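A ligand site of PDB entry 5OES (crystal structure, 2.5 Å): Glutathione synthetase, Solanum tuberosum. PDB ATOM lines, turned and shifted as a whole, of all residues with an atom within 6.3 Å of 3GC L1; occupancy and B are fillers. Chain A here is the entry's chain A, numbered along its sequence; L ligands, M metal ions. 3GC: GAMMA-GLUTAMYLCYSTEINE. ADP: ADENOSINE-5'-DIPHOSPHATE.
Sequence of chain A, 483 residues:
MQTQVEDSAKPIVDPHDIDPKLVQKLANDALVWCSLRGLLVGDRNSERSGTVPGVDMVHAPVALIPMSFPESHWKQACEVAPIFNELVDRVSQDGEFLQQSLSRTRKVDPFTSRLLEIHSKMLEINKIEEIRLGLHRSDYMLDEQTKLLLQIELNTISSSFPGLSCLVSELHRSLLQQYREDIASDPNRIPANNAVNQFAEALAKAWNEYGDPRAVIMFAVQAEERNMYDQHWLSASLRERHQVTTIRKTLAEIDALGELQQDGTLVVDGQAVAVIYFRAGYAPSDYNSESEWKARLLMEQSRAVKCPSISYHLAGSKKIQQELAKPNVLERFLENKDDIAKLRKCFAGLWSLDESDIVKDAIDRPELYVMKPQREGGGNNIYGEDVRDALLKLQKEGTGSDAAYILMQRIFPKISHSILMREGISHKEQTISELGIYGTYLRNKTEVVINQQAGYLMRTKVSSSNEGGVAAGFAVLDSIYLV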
ATOM      1  N   ARG A 137     -15.905  20.096  14.185  1.00  0.00           N
ATOM      2  CA  ARG A 137     -16.675  20.266  15.414  1.00  0.00           C
ATOM      3  C   ARG A 137     -16.567  21.711  15.879  1.00  0.00           C
ATOM      4  O   ARG A 137     -15.452  22.228  16.051  1.00  0.00           O
ATOM      5  CB  ARG A 137     -16.207  19.339  16.519  1.00  0.00           C
ATOM      6  CG  ARG A 137     -17.277  19.152  17.586  1.00  0.00           C
ATOM      7  CD  ARG A 137     -16.788  18.337  18.768  1.00  0.00           C
ATOM      8  NE  ARG A 137     -15.738  19.052  19.478  1.00  0.00           N
ATOM      9  CZ  ARG A 137     -14.474  18.648  19.632  1.00  0.00           C
ATOM     10  NH1 ARG A 137     -14.041  17.482  19.181  1.00  0.00           N
ATOM     11  NH2 ARG A 137     -13.634  19.442  20.292  1.00  0.00           N
ATOM     12  N   ASP A 139     -17.319  24.245  18.885  1.00  0.00           N
ATOM     13  CA  ASP A 139     -17.443  24.175  20.340  1.00  0.00           C
ATOM     14  C   ASP A 139     -18.007  25.465  20.923  1.00  0.00           C
ATOM     15  O   ASP A 139     -17.552  26.553  20.578  1.00  0.00           O
ATOM     16  CB  ASP A 139     -16.090  23.849  20.969  1.00  0.00           C
ATOM     17  CG  ASP A 139     -15.639  22.417  20.670  1.00  0.00           C
ATOM     18  OD1 ASP A 139     -16.465  21.475  20.749  1.00  0.00           O
ATOM     19  OD2 ASP A 139     -14.432  22.242  20.385  1.00  0.00           O
ATOM     20  N   GLU A 153     -14.333  27.615  19.891  1.00  0.00           N
ATOM     21  CA  GLU A 153     -13.477  27.330  18.743  1.00  0.00           C
ATOM     22  C   GLU A 153     -14.139  26.522  17.652  1.00  0.00           C
ATOM     23  O   GLU A 153     -15.228  25.992  17.835  1.00  0.00           O
ATOM     24  CB  GLU A 153     -12.180  26.635  19.180  1.00  0.00           C
ATOM     25  CG  GLU A 153     -12.382  25.346  19.934  1.00  0.00           C
ATOM     26  CD  GLU A 153     -11.085  24.602  20.149  1.00  0.00           C
ATOM     27  OE1 GLU A 153     -10.013  25.203  19.942  1.00  0.00           O
ATOM     28  OE2 GLU A 153     -11.146  23.381  20.458  1.00  0.00           O
ATOM     29  N   ASN A 155     -12.933  23.364  15.224  1.00  0.00           N
ATOM     30  CA  ASN A 155     -11.941  22.329  14.911  1.00  0.00           C
ATOM     31  C   ASN A 155     -12.107  21.845  13.493  1.00  0.00           C
ATOM     32  O   ASN A 155     -13.155  21.307  13.161  1.00  0.00           O
ATOM     33  CB  ASN A 155     -12.059  21.143  15.860  1.00  0.00           C
ATOM     34  CG  ASN A 155     -11.777  21.511  17.284  1.00  0.00           C
ATOM     35  OD1 ASN A 155     -10.617  21.539  17.699  1.00  0.00           O
ATOM     36  ND2 ASN A 155     -12.831  21.793  18.042  1.00  0.00           N
ATOM     37  N   ILE A 157      -9.470  19.829  12.319  1.00  0.00           N
ATOM     38  CA  ILE A 157      -8.563  18.678  12.289  1.00  0.00           C
ATOM     39  C   ILE A 157      -8.757  17.795  13.505  1.00  0.00           C
ATOM     40  O   ILE A 157      -8.819  18.282  14.642  1.00  0.00           O
ATOM     41  CB  ILE A 157      -7.079  19.099  12.172  1.00  0.00           C
ATOM     42  CG1 ILE A 157      -6.179  17.858  12.081  1.00  0.00           C
ATOM     43  CG2 ILE A 157      -6.621  20.014  13.293  1.00  0.00           C
ATOM     44  CD1 ILE A 157      -4.833  18.135  11.420  1.00  0.00           C
ATOM     45  N   SER A 158      -8.865  16.483  13.248  1.00  0.00           N
ATOM     46  CA  SER A 158      -8.908  15.463  14.287  1.00  0.00           C
ATOM     47  C   SER A 158      -9.967  15.709  15.355  1.00  0.00           C
ATOM     48  O   SER A 158      -9.681  15.678  16.555  1.00  0.00           O
ATOM     49  CB  SER A 158      -7.524  15.307  14.947  1.00  0.00           C
ATOM     50  OG  SER A 158      -7.498  14.209  15.837  1.00  0.00           O
ATOM     51  N   SER A 159     -11.204  15.948  14.903  1.00  0.00           N
ATOM     52  CA  SER A 159     -12.326  16.186  15.804  1.00  0.00           C
ATOM     53  C   SER A 159     -12.683  14.911  16.550  1.00  0.00           C
ATOM     54  O   SER A 159     -13.219  13.966  15.959  1.00  0.00           O
ATOM     55  CB  SER A 159     -13.531  16.706  15.031  1.00  0.00           C
ATOM     56  OG  SER A 159     -13.189  17.859  14.267  1.00  0.00           O
ATOM     57  N   SER A 160     -12.337  14.875  17.838  1.00  0.00           N
ATOM     58  CA  SER A 160     -12.539  13.694  18.681  1.00  0.00           C
ATOM     59  C   SER A 160     -13.993  13.429  19.051  1.00  0.00           C
ATOM     60  O   SER A 160     -14.824  14.345  19.086  1.00  0.00           O
ATOM     61  CB  SER A 160     -11.772  13.827  19.993  1.00  0.00           C
ATOM     62  OG  SER A 160     -10.404  14.032  19.738  1.00  0.00           O
ATOM     63  N   PHE A 161     -14.247  12.151  19.317  1.00  0.00           N
ATOM     64  CA  PHE A 161     -15.455  11.639  19.967  1.00  0.00           C
ATOM     65  C   PHE A 161     -16.742  11.435  19.143  1.00  0.00           C
ATOM     66  O   PHE A 161     -17.792  11.189  19.741  1.00  0.00           O
ATOM     67  CB  PHE A 161     -15.727  12.410  21.267  1.00  0.00           C
ATOM     68  CG  PHE A 161     -14.567  12.424  22.222  1.00  0.00           C
ATOM     69  CD1 PHE A 161     -14.063  11.227  22.743  1.00  0.00           C
ATOM     70  CD2 PHE A 161     -13.995  13.634  22.621  1.00  0.00           C
ATOM     71  CE1 PHE A 161     -12.995  11.251  23.639  1.00  0.00           C
ATOM     72  CE2 PHE A 161     -12.928  13.642  23.500  1.00  0.00           C
ATOM     73  CZ  PHE A 161     -12.428  12.452  24.027  1.00  0.00           C
ATOM     74  N   GLN A 222      -1.693   8.467  15.849  1.00  0.00           N
ATOM     75  CA  GLN A 222      -0.536   8.603  16.730  1.00  0.00           C
ATOM     76  C   GLN A 222       0.029   7.242  17.093  1.00  0.00           C
ATOM     77  O   GLN A 222      -0.689   6.242  17.038  1.00  0.00           O
ATOM     78  CB  GLN A 222      -0.906   9.380  17.994  1.00  0.00           C
ATOM     79  CG  GLN A 222      -1.458  10.747  17.630  1.00  0.00           C
ATOM     80  CD  GLN A 222      -1.519  11.692  18.784  1.00  0.00           C
ATOM     81  OE1 GLN A 222      -1.746  11.284  19.944  1.00  0.00           O
ATOM     82  NE2 GLN A 222      -1.369  12.990  18.474  1.00  0.00           N
ATOM     83  N   GLU A 225      -2.141   5.671  21.327  1.00  0.00           N
ATOM     84  CA  GLU A 225      -3.483   6.234  21.267  1.00  0.00           C
ATOM     85  C   GLU A 225      -4.476   5.511  22.176  1.00  0.00           C
ATOM     86  O   GLU A 225      -5.078   4.504  21.776  1.00  0.00           O
ATOM     87  CB  GLU A 225      -3.973   6.233  19.819  1.00  0.00           C
ATOM     88  CG  GLU A 225      -5.279   6.960  19.565  1.00  0.00           C
ATOM     89  CD  GLU A 225      -5.279   8.392  20.094  1.00  0.00           C
ATOM     90  OE1 GLU A 225      -5.776   8.570  21.221  1.00  0.00           O
ATOM     91  OE2 GLU A 225      -4.740   9.306  19.406  1.00  0.00           O
ATOM     92  N   ASN A 227      -7.292   6.673  23.021  1.00  0.00           N
ATOM     93  CA  ASN A 227      -8.628   6.883  22.467  1.00  0.00           C
ATOM     94  C   ASN A 227      -8.836   6.139  21.130  1.00  0.00           C
ATOM     95  O   ASN A 227      -9.599   6.589  20.275  1.00  0.00           O
ATOM     96  CB  ASN A 227      -8.880   8.391  22.326  1.00  0.00           C
ATOM     97  CG  ASN A 227     -10.352   8.730  22.251  1.00  0.00           C
ATOM     98  OD1 ASN A 227     -11.190   8.090  22.899  1.00  0.00           O
ATOM     99  ND2 ASN A 227     -10.674   9.748  21.441  1.00  0.00           N
ATOM    100  N   ASP A 230     -12.652   5.028  19.954  1.00  0.00           N
ATOM    101  CA  ASP A 230     -13.369   6.100  19.245  1.00  0.00           C
ATOM    102  C   ASP A 230     -13.112   6.095  17.741  1.00  0.00           C
ATOM    103  O   ASP A 230     -14.040   6.230  16.930  1.00  0.00           O
ATOM    104  CB  ASP A 230     -12.959   7.456  19.837  1.00  0.00           C
ATOM    105  CG  ASP A 230     -13.752   8.618  19.253  1.00  0.00           C
ATOM    106  OD1 ASP A 230     -14.995   8.542  19.172  1.00  0.00           O
ATOM    107  OD2 ASP A 230     -13.118   9.637  18.881  1.00  0.00           O
ATOM    108  N   GLN A 231     -11.840   5.942  17.367  1.00  0.00           N
ATOM    109  CA  GLN A 231     -11.424   5.904  15.966  1.00  0.00           C
ATOM    110  C   GLN A 231     -11.892   4.602  15.287  1.00  0.00           C
ATOM    111  O   GLN A 231     -12.390   4.624  14.155  1.00  0.00           O
ATOM    112  CB  GLN A 231      -9.903   6.008  15.855  1.00  0.00           C
ATOM    113  CG  GLN A 231      -9.327   7.336  16.388  1.00  0.00           C
ATOM    114  CD  GLN A 231      -7.810   7.310  16.498  1.00  0.00           C
ATOM    115  OE1 GLN A 231      -7.193   6.327  16.125  1.00  0.00           O
ATOM    116  NE2 GLN A 231      -7.223   8.391  16.990  1.00  0.00           N
ATOM    117  N   PHE A 278      -7.213  12.557   9.196  1.00  0.00           N
ATOM    118  CA  PHE A 278      -6.175  12.842  10.178  1.00  0.00           C
ATOM    119  C   PHE A 278      -6.682  12.741  11.597  1.00  0.00           C
ATOM    120  O   PHE A 278      -7.640  13.412  11.949  1.00  0.00           O
ATOM    121  CB  PHE A 278      -5.595  14.245   9.979  1.00  0.00           C
ATOM    122  CG  PHE A 278      -4.646  14.350   8.819  1.00  0.00           C
ATOM    123  CD1 PHE A 278      -5.109  14.627   7.548  1.00  0.00           C
ATOM    124  CD2 PHE A 278      -3.290  14.154   9.007  1.00  0.00           C
ATOM    125  CE1 PHE A 278      -4.232  14.724   6.469  1.00  0.00           C
ATOM    126  CE2 PHE A 278      -2.404  14.253   7.951  1.00  0.00           C
ATOM    127  CZ  PHE A 278      -2.879  14.538   6.679  1.00  0.00           C
ATOM    128  N   ARG A 279      -6.037  11.897  12.394  1.00  0.00           N
ATOM    129  CA  ARG A 279      -6.192  11.880  13.844  1.00  0.00           C
ATOM    130  C   ARG A 279      -4.815  12.045  14.491  1.00  0.00           C
ATOM    131  O   ARG A 279      -4.506  11.478  15.556  1.00  0.00           O
ATOM    132  CB  ARG A 279      -6.897  10.596  14.285  1.00  0.00           C
ATOM    133  CG  ARG A 279      -8.307  10.439  13.700  1.00  0.00           C
ATOM    134  CD  ARG A 279      -9.279  11.447  14.288  1.00  0.00           C
ATOM    135  NE  ARG A 279      -9.618  11.113  15.672  1.00  0.00           N
ATOM    136  CZ  ARG A 279     -10.741  10.537  16.102  1.00  0.00           C
ATOM    137  NH1 ARG A 279     -10.886  10.284  17.394  1.00  0.00           N
ATOM    138  NH2 ARG A 279     -11.741  10.199  15.271  1.00  0.00           N
ATOM    139  N   ALA A 280      -3.996  12.877  13.826  1.00  0.00           N
ATOM    140  CA  ALA A 280      -2.614  13.129  14.181  1.00  0.00           C
ATOM    141  C   ALA A 280      -2.110  14.276  13.281  1.00  0.00           C
ATOM    142  O   ALA A 280      -2.802  14.684  12.343  1.00  0.00           O
ATOM    143  CB  ALA A 280      -1.775  11.878  13.986  1.00  0.00           C
ATOM    144  N   TYR A 282      -1.569  17.406  14.215  1.00  0.00           N
ATOM    145  CA  TYR A 282      -2.161  18.678  14.649  1.00  0.00           C
ATOM    146  C   TYR A 282      -1.297  19.398  15.698  1.00  0.00           C
ATOM    147  O   TYR A 282      -1.576  20.538  16.020  1.00  0.00           O
ATOM    148  CB  TYR A 282      -3.600  18.478  15.204  1.00  0.00           C
ATOM    149  CG  TYR A 282      -3.708  17.433  16.296  1.00  0.00           C
ATOM    150  CD1 TYR A 282      -3.414  17.732  17.617  1.00  0.00           C
ATOM    151  CD2 TYR A 282      -4.101  16.130  15.989  1.00  0.00           C
ATOM    152  CE1 TYR A 282      -3.492  16.769  18.621  1.00  0.00           C
ATOM    153  CE2 TYR A 282      -4.189  15.151  16.971  1.00  0.00           C
ATOM    154  CZ  TYR A 282      -3.876  15.476  18.284  1.00  0.00           C
ATOM    155  OH  TYR A 282      -3.967  14.503  19.254  1.00  0.00           O
ATOM    156  N   LEU A 457     -21.445  16.627  20.874  1.00  0.00           N
ATOM    157  CA  LEU A 457     -20.621  16.230  21.986  1.00  0.00           C
ATOM    158  C   LEU A 457     -20.907  17.175  23.142  1.00  0.00           C
ATOM    159  O   LEU A 457     -20.972  18.389  22.937  1.00  0.00           O
ATOM    160  CB  LEU A 457     -19.149  16.368  21.570  1.00  0.00           C
ATOM    161  CG  LEU A 457     -18.074  16.187  22.653  1.00  0.00           C
ATOM    162  CD1 LEU A 457     -18.183  14.823  23.293  1.00  0.00           C
ATOM    163  CD2 LEU A 457     -16.699  16.388  22.050  1.00  0.00           C
ATOM    164  N   ARG A 459     -19.034  17.843  26.758  1.00  0.00           N
ATOM    165  CA  ARG A 459     -17.943  17.546  27.677  1.00  0.00           C
ATOM    166  C   ARG A 459     -18.185  18.367  28.921  1.00  0.00           C
ATOM    167  O   ARG A 459     -18.492  19.558  28.843  1.00  0.00           O
ATOM    168  CB  ARG A 459     -16.573  17.876  27.069  1.00  0.00           C
ATOM    169  CG  ARG A 459     -16.033  16.786  26.155  1.00  0.00           C
ATOM    170  CD  ARG A 459     -14.748  17.189  25.411  1.00  0.00           C
ATOM    171  NE  ARG A 459     -14.881  18.523  24.811  1.00  0.00           N
ATOM    172  CZ  ARG A 459     -14.006  19.087  23.991  1.00  0.00           C
ATOM    173  NH1 ARG A 459     -12.910  18.432  23.570  1.00  0.00           N
ATOM    174  NH2 ARG A 459     -14.257  20.318  23.551  1.00  0.00           N
HETATM  175  N1  3GC L   1      -5.369  12.068  19.099  1.00  0.00           N
HETATM  176  CA1 3GC L   1      -6.612  11.946  19.846  1.00  0.00           C
HETATM  177  C1  3GC L   1      -7.700  11.405  18.975  1.00  0.00           C
HETATM  178  O11 3GC L   1      -8.825  11.183  19.523  1.00  0.00           O
HETATM  179  O12 3GC L   1      -7.469  11.222  17.753  1.00  0.00           O
HETATM  180  CB1 3GC L   1      -7.035  13.299  20.407  1.00  0.00           C
HETATM  181  CG1 3GC L   1      -7.351  14.321  19.319  1.00  0.00           C
HETATM  182  CD1 3GC L   1      -7.840  15.633  19.917  1.00  0.00           C
HETATM  183  OE1 3GC L   1      -7.704  15.880  21.114  1.00  0.00           O
HETATM  184  N2  3GC L   1      -8.415  16.470  19.040  1.00  0.00           N
HETATM  185  CA2 3GC L   1      -8.888  17.814  19.364  1.00  0.00           C
HETATM  186  C2  3GC L   1     -10.364  17.918  19.694  1.00  0.00           C
HETATM  187  O2  3GC L   1     -11.130  16.933  19.603  1.00  0.00           O
HETATM  188  CB2 3GC L   1      -8.575  18.747  18.191  1.00  0.00           C
HETATM  189  SG2 3GC L   1      -6.868  18.600  17.630  1.00  0.00           S
HETATM  190  O3  3GC L   1     -10.777  19.032  20.062  1.00  0.00           O
HETATM  191  PB  ADP L   2      -7.565  23.662  23.552  1.00  0.00           P
HETATM  192  O1B ADP L   2      -7.236  23.474  25.028  1.00  0.00           O
HETATM  193  O2B ADP L   2      -6.322  23.673  22.682  1.00  0.00           O
HETATM  194  O3B ADP L   2      -8.663  22.761  23.021  1.00  0.00           O
HETATM  195  PA  ADP L   2      -9.629  25.741  23.810  1.00  0.00           P
HETATM  196  O1A ADP L   2     -10.694  24.685  23.566  1.00  0.00           O
HETATM  197  O2A ADP L   2      -9.835  27.057  23.090  1.00  0.00           O
HETATM  198  O3A ADP L   2      -8.152  25.172  23.396  1.00  0.00           O
HETATM  199  O5' ADP L   2      -9.453  26.013  25.410  1.00  0.00           O
HETATM  200  C5' ADP L   2      -9.480  24.989  26.426  1.00  0.00           C
HETATM  201  C4' ADP L   2     -10.550  25.243  27.494  1.00  0.00           C
HETATM  202  O4' ADP L   2     -10.486  26.581  27.997  1.00  0.00           O
HETATM  203  C3' ADP L   2     -11.979  25.081  26.984  1.00  0.00           C
HETATM  204  O3' ADP L   2     -12.461  23.745  27.085  1.00  0.00           O
HETATM  205  C2' ADP L   2     -12.805  26.029  27.846  1.00  0.00           C
HETATM  206  O2' ADP L   2     -13.326  25.416  29.028  1.00  0.00           O
HETATM  207  C1' ADP L   2     -11.802  27.111  28.225  1.00  0.00           C
HETATM  208  N9  ADP L   2     -12.062  28.315  27.405  1.00  0.00           N
HETATM  209  C8  ADP L   2     -11.669  28.540  26.129  1.00  0.00           C
HETATM  210  N7  ADP L   2     -12.074  29.751  25.695  1.00  0.00           N
HETATM  211  C5  ADP L   2     -12.758  30.313  26.703  1.00  0.00           C
HETATM  212  C6  ADP L   2     -13.469  31.590  26.909  1.00  0.00           C
HETATM  213  N6  ADP L   2     -13.513  32.516  25.919  1.00  0.00           N
HETATM  214  N1  ADP L   2     -14.039  31.782  28.121  1.00  0.00           N
HETATM  215  C2  ADP L   2     -13.987  30.856  29.117  1.00  0.00           C
HETATM  216  N3  ADP L   2     -13.363  29.687  28.982  1.00  0.00           N
HETATM  217  C4  ADP L   2     -12.747  29.366  27.823  1.00  0.00           C
HETATM  218 MG    MG M   1     -12.590  23.109  22.713  1.00  0.00          MG
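OH of Tyr 282 lies within hydrogen-bond range of NE2 of Gln 222, at 3.1 Å. The side-chain carboxylate of Glu 225 sits at hydrogen-bond distance from the backbone NH of Asn 227 (3.0 Å). The backbone carbonyl oxygen (O) of Ser 160 sits at hydrogen-bond distance from the guanidinium group (NH1) of Arg 137 (3.2 Å). The backbone carbonyl oxygen (O) of Arg 137 lies within hydrogen-bond range of the backbone NH (N) of Asn 155, at 2.9 Å. NE of Arg 137 is in salt-bridge range of OD1 of Asp 139 (2.8 Å). The guanidinium group of Arg 279 is in salt-bridge range of the side-chain carboxylate of Asp 230 (2.8 Å). The side-chain amide nitrogen (ND2) of Asn 155 sits at hydrogen-bond distance from the side-chain carboxylate (OE2) of Glu 153, at 3.3 Å. The side-chain amide nitrogen of Asn 155 is in hydrogen-bond range of the side-chain carboxylate of Asp 139 (2.9 Å).
N1 of 3GC L1 lies within hydrogen-bond range of OH of Tyr 282, 2.8 Å away. A nitrogen (N1) of 3GC L1 is in salt-bridge range of the side-chain carboxylate (OE2) of Glu 225 (2.8 Å). NH2 of Arg 137 is in salt-bridge range of O3 of 3GC L1, at 2.9 Å. The backbone carbonyl oxygen (O) of Ser 158 lies within hydrogen-bond range of a nitrogen (N2) of 3GC L1 (2.9 Å). An oxygen (O12) of 3GC L1 sits at hydrogen-bond distance from the side-chain amide nitrogen (NE2) of Gln 231 (2.9 Å). The backbone NH (N) of Ser 160 sits at hydrogen-bond distance from an oxygen (O2) of 3GC L1 (3.0 Å). The side-chain hydroxyl (OG) of Ser 160 sits at hydrogen-bond distance from an oxygen (O2) of 3GC L1 (3.0 Å). O12 of 3GC L1 is in salt-bridge range of NE of Arg 279 (3.0 Å). An oxygen (O11) of 3GC L1 lies within hydrogen-bond range of the side-chain amide nitrogen (ND2) of Asn 227 (3.0 Å). An oxygen (O3) of 3GC L1 sits close to the side-chain amide oxygen (OD1) of Asn 155. A sulfur (SG2) of 3GC L1 lies close to the backbone carbonyl oxygen of Ile 157 (3.6 Å).
C of Ser 159 touches O2 of 3GC L1 (3.98 Å). Gln 222 touches 3GC L1 (OE1 to N1, 3.8 Å). Hydrophobic or aromatic side chains within 4 Å of 3GC L1: Tyr 282. Of the 20 residues printed, 12 come within 4 Å of 3GC L1.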
